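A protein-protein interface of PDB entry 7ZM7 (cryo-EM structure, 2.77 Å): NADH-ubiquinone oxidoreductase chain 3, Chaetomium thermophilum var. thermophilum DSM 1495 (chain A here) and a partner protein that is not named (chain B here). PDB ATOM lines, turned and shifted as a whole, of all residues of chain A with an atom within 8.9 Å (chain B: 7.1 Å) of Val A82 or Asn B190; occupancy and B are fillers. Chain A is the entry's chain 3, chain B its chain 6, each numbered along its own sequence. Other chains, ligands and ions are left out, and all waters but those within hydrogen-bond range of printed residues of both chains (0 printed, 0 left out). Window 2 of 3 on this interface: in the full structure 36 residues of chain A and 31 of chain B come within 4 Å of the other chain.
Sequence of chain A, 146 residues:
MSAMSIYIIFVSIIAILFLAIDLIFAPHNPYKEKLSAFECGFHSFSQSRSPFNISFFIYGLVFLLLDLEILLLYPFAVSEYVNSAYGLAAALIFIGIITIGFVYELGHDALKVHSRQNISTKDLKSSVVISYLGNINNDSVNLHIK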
ATOM      1  N   PRO A  75      26.855  12.626  -5.644  1.00  0.00           N
ATOM      2  CA  PRO A  75      26.083  13.282  -6.702  1.00  0.00           C
ATOM      3  C   PRO A  75      24.998  14.197  -6.188  1.00  0.00           C
ATOM      4  O   PRO A  75      24.700  15.200  -6.837  1.00  0.00           O
ATOM      5  CB  PRO A  75      25.511  12.097  -7.488  1.00  0.00           C
ATOM      6  CG  PRO A  75      26.427  11.011  -7.236  1.00  0.00           C
ATOM      7  CD  PRO A  75      26.867  11.168  -5.837  1.00  0.00           C
ATOM      8  N   PHE A  76      24.398  13.893  -5.041  1.00  0.00           N
ATOM      9  CA  PHE A  76      23.366  14.766  -4.500  1.00  0.00           C
ATOM     10  C   PHE A  76      23.926  16.127  -4.129  1.00  0.00           C
ATOM     11  O   PHE A  76      23.286  17.152  -4.369  1.00  0.00           O
ATOM     12  CB  PHE A  76      22.708  14.127  -3.283  1.00  0.00           C
ATOM     13  CG  PHE A  76      21.635  14.967  -2.691  1.00  0.00           C
ATOM     14  CD1 PHE A  76      20.399  15.027  -3.277  1.00  0.00           C
ATOM     15  CD2 PHE A  76      21.879  15.736  -1.572  1.00  0.00           C
ATOM     16  CE1 PHE A  76      19.437  15.818  -2.761  1.00  0.00           C
ATOM     17  CE2 PHE A  76      20.908  16.533  -1.056  1.00  0.00           C
ATOM     18  CZ  PHE A  76      19.682  16.570  -1.651  1.00  0.00           C
ATOM     19  N   ALA A  77      25.114  16.162  -3.535  1.00  0.00           N
ATOM     20  CA  ALA A  77      25.687  17.429  -3.028  1.00  0.00           C
ATOM     21  C   ALA A  77      26.087  18.377  -4.162  1.00  0.00           C
ATOM     22  O   ALA A  77      26.169  19.584  -3.906  1.00  0.00           O
ATOM     23  CB  ALA A  77      26.845  17.103  -2.141  1.00  0.00           C
ATOM     24  N   VAL A  78      26.269  17.856  -5.370  1.00  0.00           N
ATOM     25  CA  VAL A  78      26.663  18.694  -6.534  1.00  0.00           C
ATOM     26  C   VAL A  78      25.458  18.832  -7.461  1.00  0.00           C
ATOM     27  O   VAL A  78      25.651  19.239  -8.600  1.00  0.00           O
ATOM     28  CB  VAL A  78      27.914  18.137  -7.240  1.00  0.00           C
ATOM     29  CG1 VAL A  78      29.166  18.287  -6.397  1.00  0.00           C
ATOM     30  CG2 VAL A  78      27.733  16.696  -7.676  1.00  0.00           C
ATOM     31  N   SER A  79      24.273  18.449  -6.997  1.00  0.00           N
ATOM     32  CA  SER A  79      23.033  18.587  -7.804  1.00  0.00           C
ATOM     33  C   SER A  79      21.882  19.108  -6.947  1.00  0.00           C
ATOM     34  O   SER A  79      20.746  18.970  -7.385  1.00  0.00           O
ATOM     35  CB  SER A  79      22.677  17.289  -8.466  1.00  0.00           C
ATOM     36  OG  SER A  79      22.195  16.342  -7.529  1.00  0.00           O
ATOM     37  N   GLU A  80      22.175  19.664  -5.770  1.00  0.00           N
ATOM     38  CA  GLU A  80      21.140  20.117  -4.791  1.00  0.00           C
ATOM     39  C   GLU A  80      20.138  21.129  -5.339  1.00  0.00           C
ATOM     40  O   GLU A  80      18.949  20.967  -5.039  1.00  0.00           O
ATOM     41  CB  GLU A  80      21.804  20.666  -3.529  1.00  0.00           C
ATOM     42  CG  GLU A  80      22.183  19.590  -2.535  1.00  0.00           C
ATOM     43  CD  GLU A  80      23.161  20.046  -1.470  1.00  0.00           C
ATOM     44  OE1 GLU A  80      23.753  21.125  -1.647  1.00  0.00           O
ATOM     45  OE2 GLU A  80      23.321  19.327  -0.466  1.00  0.00           O
ATOM     46  N   TYR A  81      20.592  22.149  -6.063  1.00  0.00           N
ATOM     47  CA  TYR A  81      19.677  23.234  -6.498  1.00  0.00           C
ATOM     48  C   TYR A  81      18.553  22.684  -7.378  1.00  0.00           C
ATOM     49  O   TYR A  81      17.394  23.056  -7.162  1.00  0.00           O
ATOM     50  CB  TYR A  81      20.478  24.276  -7.282  1.00  0.00           C
ATOM     51  CG  TYR A  81      19.748  25.556  -7.591  1.00  0.00           C
ATOM     52  CD1 TYR A  81      19.681  26.577  -6.660  1.00  0.00           C
ATOM     53  CD2 TYR A  81      19.130  25.751  -8.815  1.00  0.00           C
ATOM     54  CE1 TYR A  81      19.015  27.758  -6.934  1.00  0.00           C
ATOM     55  CE2 TYR A  81      18.456  26.924  -9.103  1.00  0.00           C
ATOM     56  CZ  TYR A  81      18.400  27.932  -8.158  1.00  0.00           C
ATOM     57  OH  TYR A  81      17.740  29.094  -8.427  1.00  0.00           O
ATOM     58  N   VAL A  82      18.886  21.841  -8.350  1.00  0.00           N
ATOM     59  CA  VAL A  82      17.847  21.209  -9.215  1.00  0.00           C
ATOM     60  C   VAL A  82      17.030  20.208  -8.397  1.00  0.00           C
ATOM     61  O   VAL A  82      15.800  20.208  -8.541  1.00  0.00           O
ATOM     62  CB  VAL A  82      18.470  20.565 -10.468  1.00  0.00           C
ATOM     63  CG1 VAL A  82      17.584  19.494 -11.083  1.00  0.00           C
ATOM     64  CG2 VAL A  82      18.861  21.609 -11.500  1.00  0.00           C
ATOM     65  N   ASN A  83      17.687  19.411  -7.554  1.00  0.00           N
ATOM     66  CA  ASN A  83      16.962  18.340  -6.829  1.00  0.00           C
ATOM     67  C   ASN A  83      15.910  18.990  -5.943  1.00  0.00           C
ATOM     68  O   ASN A  83      14.770  18.489  -5.938  1.00  0.00           O
ATOM     69  CB  ASN A  83      17.931  17.459  -6.037  1.00  0.00           C
ATOM     70  CG  ASN A  83      18.509  16.321  -6.850  1.00  0.00           C
ATOM     71  OD1 ASN A  83      19.575  15.804  -6.531  1.00  0.00           O
ATOM     72  ND2 ASN A  83      17.817  15.926  -7.906  1.00  0.00           N
ATOM     73  N   SER A  84      16.282  20.057  -5.231  1.00  0.00           N
ATOM     74  CA  SER A  84      15.330  20.823  -4.389  1.00  0.00           C
ATOM     75  C   SER A  84      14.636  19.930  -3.364  1.00  0.00           C
ATOM     76  O   SER A  84      15.286  19.012  -2.843  1.00  0.00           O
ATOM     77  CB  SER A  84      14.334  21.574  -5.231  1.00  0.00           C
ATOM     78  OG  SER A  84      13.715  22.606  -4.478  1.00  0.00           O
ATOM     79  N   ALA A  85      13.355  20.195  -3.106  1.00  0.00           N
ATOM     80  CA  ALA A  85      12.596  19.455  -2.078  1.00  0.00           C
ATOM     81  C   ALA A  85      12.407  17.982  -2.452  1.00  0.00           C
ATOM     82  O   ALA A  85      12.562  17.137  -1.559  1.00  0.00           O
ATOM     83  CB  ALA A  85      11.274  20.146  -1.917  1.00  0.00           C
ATOM     84  N   TYR A  86      12.059  17.692  -3.710  1.00  0.00           N
ATOM     85  CA  TYR A  86      11.774  16.292  -4.114  1.00  0.00           C
ATOM     86  C   TYR A  86      13.043  15.452  -4.005  1.00  0.00           C
ATOM     87  O   TYR A  86      12.972  14.328  -3.484  1.00  0.00           O
ATOM     88  CB  TYR A  86      11.119  16.255  -5.497  1.00  0.00           C
ATOM     89  CG  TYR A  86      10.453  14.952  -5.854  1.00  0.00           C
ATOM     90  CD1 TYR A  86       9.202  14.630  -5.360  1.00  0.00           C
ATOM     91  CD2 TYR A  86      11.074  14.045  -6.695  1.00  0.00           C
ATOM     92  CE1 TYR A  86       8.586  13.433  -5.685  1.00  0.00           C
ATOM     93  CE2 TYR A  86      10.474  12.846  -7.033  1.00  0.00           C
ATOM     94  CZ  TYR A  86       9.226  12.541  -6.527  1.00  0.00           C
ATOM     95  OH  TYR A  86       8.634  11.360  -6.859  1.00  0.00           O
ATOM     96  N   GLY A  87      14.169  15.992  -4.470  1.00  0.00           N
ATOM     97  CA  GLY A  87      15.452  15.275  -4.375  1.00  0.00           C
ATOM     98  C   GLY A  87      15.857  15.091  -2.933  1.00  0.00           C
ATOM     99  O   GLY A  87      16.376  14.019  -2.605  1.00  0.00           O
ATOM    100  N   LEU A  88      15.643  16.122  -2.111  1.00  0.00           N
ATOM    101  CA  LEU A  88      15.981  16.041  -0.671  1.00  0.00           C
ATOM    102  C   LEU A  88      15.197  14.885  -0.058  1.00  0.00           C
ATOM    103  O   LEU A  88      15.818  14.064   0.624  1.00  0.00           O
ATOM    104  CB  LEU A  88      15.626  17.368   0.000  1.00  0.00           C
ATOM    105  CG  LEU A  88      15.949  17.469   1.489  1.00  0.00           C
ATOM    106  CD1 LEU A  88      17.434  17.272   1.739  1.00  0.00           C
ATOM    107  CD2 LEU A  88      15.488  18.805   2.049  1.00  0.00           C
ATOM    108  N   ASN B 182      26.771  20.769 -17.324  1.00  0.00           N
ATOM    109  CA  ASN B 182      26.941  20.109 -16.016  1.00  0.00           C
ATOM    110  C   ASN B 182      28.002  19.032 -16.163  1.00  0.00           C
ATOM    111  O   ASN B 182      28.109  18.462 -17.258  1.00  0.00           O
ATOM    112  CB  ASN B 182      25.629  19.518 -15.498  1.00  0.00           C
ATOM    113  CG  ASN B 182      24.497  20.516 -15.421  1.00  0.00           C
ATOM    114  OD1 ASN B 182      24.717  21.711 -15.237  1.00  0.00           O
ATOM    115  ND2 ASN B 182      23.276  20.029 -15.551  1.00  0.00           N
ATOM    116  N   ASN B 183      28.775  18.802 -15.106  1.00  0.00           N
ATOM    117  CA  ASN B 183      29.736  17.677 -15.118  1.00  0.00           C
ATOM    118  C   ASN B 183      28.910  16.393 -15.072  1.00  0.00           C
ATOM    119  O   ASN B 183      27.749  16.465 -14.656  1.00  0.00           O
ATOM    120  CB  ASN B 183      30.692  17.773 -13.934  1.00  0.00           C
ATOM    121  CG  ASN B 183      31.528  19.032 -13.951  1.00  0.00           C
ATOM    122  OD1 ASN B 183      32.065  19.409 -14.989  1.00  0.00           O
ATOM    123  ND2 ASN B 183      31.650  19.680 -12.804  1.00  0.00           N
ATOM    124  N   HIS B 184      29.482  15.263 -15.456  1.00  0.00           N
ATOM    125  CA  HIS B 184      28.700  14.003 -15.515  1.00  0.00           C
ATOM    126  C   HIS B 184      28.071  13.684 -14.161  1.00  0.00           C
ATOM    127  O   HIS B 184      26.980  13.120 -14.186  1.00  0.00           O
ATOM    128  CB  HIS B 184      29.536  12.817 -15.997  1.00  0.00           C
ATOM    129  CG  HIS B 184      30.046  12.925 -17.393  1.00  0.00           C
ATOM    130  ND1 HIS B 184      31.224  12.333 -17.793  1.00  0.00           N
ATOM    131  CD2 HIS B 184      29.548  13.542 -18.482  1.00  0.00           C
ATOM    132  CE1 HIS B 184      31.429  12.580 -19.067  1.00  0.00           C
ATOM    133  NE2 HIS B 184      30.419  13.320 -19.511  1.00  0.00           N
ATOM    134  N   ILE B 185      28.696  14.059 -13.036  1.00  0.00           N
ATOM    135  CA  ILE B 185      28.168  13.656 -11.704  1.00  0.00           C
ATOM    136  C   ILE B 185      26.940  14.516 -11.384  1.00  0.00           C
ATOM    137  O   ILE B 185      26.017  13.989 -10.758  1.00  0.00           O
ATOM    138  CB  ILE B 185      29.286  13.841 -10.663  1.00  0.00           C
ATOM    139  CG1 ILE B 185      28.835  13.428  -9.258  1.00  0.00           C
ATOM    140  CG2 ILE B 185      29.866  15.248 -10.689  1.00  0.00           C
ATOM    141  CD1 ILE B 185      29.865  13.648  -8.186  1.00  0.00           C
ATOM    142  N   SER B 186      26.927  15.783 -11.788  1.00  0.00           N
ATOM    143  CA  SER B 186      25.737  16.640 -11.606  1.00  0.00           C
ATOM    144  C   SER B 186      24.601  16.164 -12.498  1.00  0.00           C
ATOM    145  O   SER B 186      23.465  16.200 -12.039  1.00  0.00           O
ATOM    146  CB  SER B 186      26.107  18.054 -11.851  1.00  0.00           C
ATOM    147  OG  SER B 186      27.112  18.467 -10.938  1.00  0.00           O
ATOM    148  N   SER B 187      24.910  15.746 -13.720  1.00  0.00           N
ATOM    149  CA  SER B 187      23.882  15.166 -14.613  1.00  0.00           C
ATOM    150  C   SER B 187      23.320  13.860 -14.024  1.00  0.00           C
ATOM    151  O   SER B 187      22.102  13.687 -14.092  1.00  0.00           O
ATOM    152  CB  SER B 187      24.452  15.004 -15.979  1.00  0.00           C
ATOM    153  OG  SER B 187      25.220  16.138 -16.329  1.00  0.00           O
ATOM    154  N   ILE B 188      24.164  12.991 -13.464  1.00  0.00           N
ATOM    155  CA  ILE B 188      23.711  11.737 -12.794  1.00  0.00           C
ATOM    156  C   ILE B 188      22.868  12.148 -11.595  1.00  0.00           C
ATOM    157  O   ILE B 188      21.808  11.581 -11.427  1.00  0.00           O
ATOM    158  CB  ILE B 188      24.911  10.850 -12.384  1.00  0.00           C
ATOM    159  CG1 ILE B 188      25.667  10.319 -13.603  1.00  0.00           C
ATOM    160  CG2 ILE B 188      24.472   9.715 -11.473  1.00  0.00           C
ATOM    161  CD1 ILE B 188      26.949   9.603 -13.271  1.00  0.00           C
ATOM    162  N   GLY B 189      23.292  13.164 -10.851  1.00  0.00           N
ATOM    163  CA  GLY B 189      22.551  13.603  -9.659  1.00  0.00           C
ATOM    164  C   GLY B 189      21.204  14.208  -9.976  1.00  0.00           C
ATOM    165  O   GLY B 189      20.279  13.943  -9.210  1.00  0.00           O
ATOM    166  N   ASN B 190      21.082  14.931 -11.092  1.00  0.00           N
ATOM    167  CA  ASN B 190      19.815  15.595 -11.489  1.00  0.00           C
ATOM    168  C   ASN B 190      18.730  14.531 -11.643  1.00  0.00           C
ATOM    169  O   ASN B 190      17.562  14.873 -11.480  1.00  0.00           O
ATOM    170  CB  ASN B 190      19.948  16.397 -12.785  1.00  0.00           C
ATOM    171  CG  ASN B 190      20.869  17.594 -12.702  1.00  0.00           C
ATOM    172  OD1 ASN B 190      21.105  18.139 -11.628  1.00  0.00           O
ATOM    173  ND2 ASN B 190      21.396  18.011 -13.841  1.00  0.00           N
ATOM    174  N   ILE B 191      19.101  13.289 -11.949  1.00  0.00           N
ATOM    175  CA  ILE B 191      18.075  12.239 -12.204  1.00  0.00           C
ATOM    176  C   ILE B 191      18.189  11.069 -11.210  1.00  0.00           C
ATOM    177  O   ILE B 191      17.193  10.348 -11.063  1.00  0.00           O
ATOM    178  CB  ILE B 191      18.151  11.792 -13.681  1.00  0.00           C
ATOM    179  CG1 ILE B 191      19.445  11.037 -13.977  1.00  0.00           C
ATOM    180  CG2 ILE B 191      17.953  12.966 -14.623  1.00  0.00           C
ATOM    181  CD1 ILE B 191      19.323  10.051 -15.101  1.00  0.00           C
ATOM    182  N   MET B 192      19.331  10.891 -10.539  1.00  0.00           N
ATOM    183  CA  MET B 192      19.534   9.731  -9.678  1.00  0.00           C
ATOM    184  C   MET B 192      18.599   9.726  -8.474  1.00  0.00           C
ATOM    185  O   MET B 192      18.285   8.661  -7.933  1.00  0.00           O
ATOM    186  CB  MET B 192      20.996   9.705  -9.242  1.00  0.00           C
ATOM    187  CG  MET B 192      21.314   8.964  -7.985  1.00  0.00           C
ATOM    188  SD  MET B 192      23.068   8.883  -7.660  1.00  0.00           S
ATOM    189  CE  MET B 192      23.065   7.433  -6.627  1.00  0.00           C
ATOM    190  N   TYR B 193      18.153  10.903  -8.029  1.00  0.00           N
ATOM    191  CA  TYR B 193      17.357  10.960  -6.776  1.00  0.00           C
ATOM    192  C   TYR B 193      15.896  11.309  -7.049  1.00  0.00           C
ATOM    193  O   TYR B 193      15.132  11.394  -6.098  1.00  0.00           O
ATOM    194  CB  TYR B 193      17.984  11.952  -5.795  1.00  0.00           C
ATOM    195  CG  TYR B 193      19.456  11.752  -5.569  1.00  0.00           C
ATOM    196  CD1 TYR B 193      19.919  10.910  -4.574  1.00  0.00           C
ATOM    197  CD2 TYR B 193      20.384  12.401  -6.361  1.00  0.00           C
ATOM    198  CE1 TYR B 193      21.273  10.716  -4.371  1.00  0.00           C
ATOM    199  CE2 TYR B 193      21.739  12.212  -6.180  1.00  0.00           C
ATOM    200  CZ  TYR B 193      22.183  11.372  -5.178  1.00  0.00           C
ATOM    201  OH  TYR B 193      23.519  11.209  -4.994  1.00  0.00           O
ATOM    202  N   THR B 194      15.518  11.507  -8.309  1.00  0.00           N
ATOM    203  CA  THR B 194      14.129  11.947  -8.628  1.00  0.00           C
ATOM    204  C   THR B 194      13.457  10.987  -9.599  1.00  0.00           C
ATOM    205  O   THR B 194      12.673  10.176  -9.139  1.00  0.00           O
ATOM    206  CB  THR B 194      14.134  13.383  -9.162  1.00  0.00           C
ATOM    207  OG1 THR B 194      15.134  13.485 -10.172  1.00  0.00           O
ATOM    208  CG2 THR B 194      14.399  14.412  -8.086  1.00  0.00           C
ATOM    209  N   ASN B 195      13.783  11.074 -10.884  1.00  0.00           N
ATOM    210  CA  ASN B 195      13.166  10.277 -11.973  1.00  0.00           C
ATOM    211  C   ASN B 195      13.396   8.775 -11.843  1.00  0.00           C
ATOM    212  O   ASN B 195      12.454   8.026 -12.100  1.00  0.00           O
ATOM    213  CB  ASN B 195      13.776  10.714 -13.303  1.00  0.00           C
ATOM    214  CG  ASN B 195      13.471  12.134 -13.721  1.00  0.00           C
ATOM    215  OD1 ASN B 195      12.782  12.348 -14.713  1.00  0.00           O
ATOM    216  ND2 ASN B 195      14.004  13.108 -13.004  1.00  0.00           N
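OH of Tyr B193 is in hydrogen-bond range of N of Phe A76 (2.8 Å).
OG of Ser B186 lies within hydrogen-bond range of O of Val A78 (2.9 Å).
O of Gly B189 sits close to OD1 of Asn A83.
O of Pro A75 lies within hydrogen-bond range of OG of Ser A79, at 2.8 Å.
The side-chain hydroxyl (OG) of Ser A79 sits at hydrogen-bond distance from the side-chain amide oxygen (OD1) of Asn A83 (2.9 Å).
The side-chain amide nitrogen (ND2) of Asn B182 sits close to the side-chain amide nitrogen (ND2) of Asn B190 (3.2 Å).
The side-chain amide oxygen of Asn B190 sits close to the backbone carbonyl oxygen of Ser B186, at 3.1 Å.
The side-chain sulfur (SD) of Met B192 sits at hydrogen-bond distance from the side-chain hydroxyl (OH) of Tyr B193 (3.6 Å).
The side-chain hydroxyl (OG1) of Thr B194 sits at hydrogen-bond distance from the side-chain amide nitrogen (ND2) of Asn B195, at 3.1 Å.
Among the printed residues, pairs that only touch across the chains: Pro A75 with Tyr B193 (3.3 Å), Ser A79 with Gly B189 (3.4 Å), Asn A83 with Tyr B193 (3.5 Å), Tyr A86 with Thr B194 (3.6 Å), Ser A79 with Asn B190 (3.6 Å), Asn A83 with Asn B190 (3.7 Å), Asn A83 with Thr B194 (3.7 Å), Val A78 with Ile B185 (3.8 Å), Pro A75 with Ile B185 (3.8 Å), Val A82 with Asn B190 (3.8 Å), Ser A79 with Ser B186 (3.8 Å), Pro A75 with Gly B189 (3.9 Å), Gly A87 with Thr B194 (3.95 Å) and Pro A75 with Met B192 (3.999 Å).
Of the printed residues of chain B, Val A78 touches Ile B185 (3.8 Å) and Ser B186 (2.9 Å).
Of the printed residues of chain A, Ile B185 touches Pro A75 and Val A78.
Ser B187 touches none of the printed residues of chain A.
Of chain A, only Pro A75 (3.9 Å), Ser A79 (3.4 Å) and Asn A83 (3.3 Å) come within 4 Å of Gly B189.
Asn B190 touches just these residues of chain A: Ser A79, Val A82 and Asn A83.
The nearest residue of chain B that does not touch Val A82 is Thr B194 (6.0 Å).
The nearest printed residue of chain A that does not touch Ser B186 is Pro A75 (5.1 Å).
Hydrophobic or aromatic side chains of chain B within 4 Å of the printed part of chain A: Ile B185, Met B192 and Tyr B193.
Along chain A the printed residues that touch a printed residue of chain B span positions 75 to 87.
Among the printed residues, 17 pairs touch across the chains.
Among the printed residues, no Asp or Glu carboxylate lies within 4 Å of a Lys or Arg side-chain nitrogen of the other chain.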
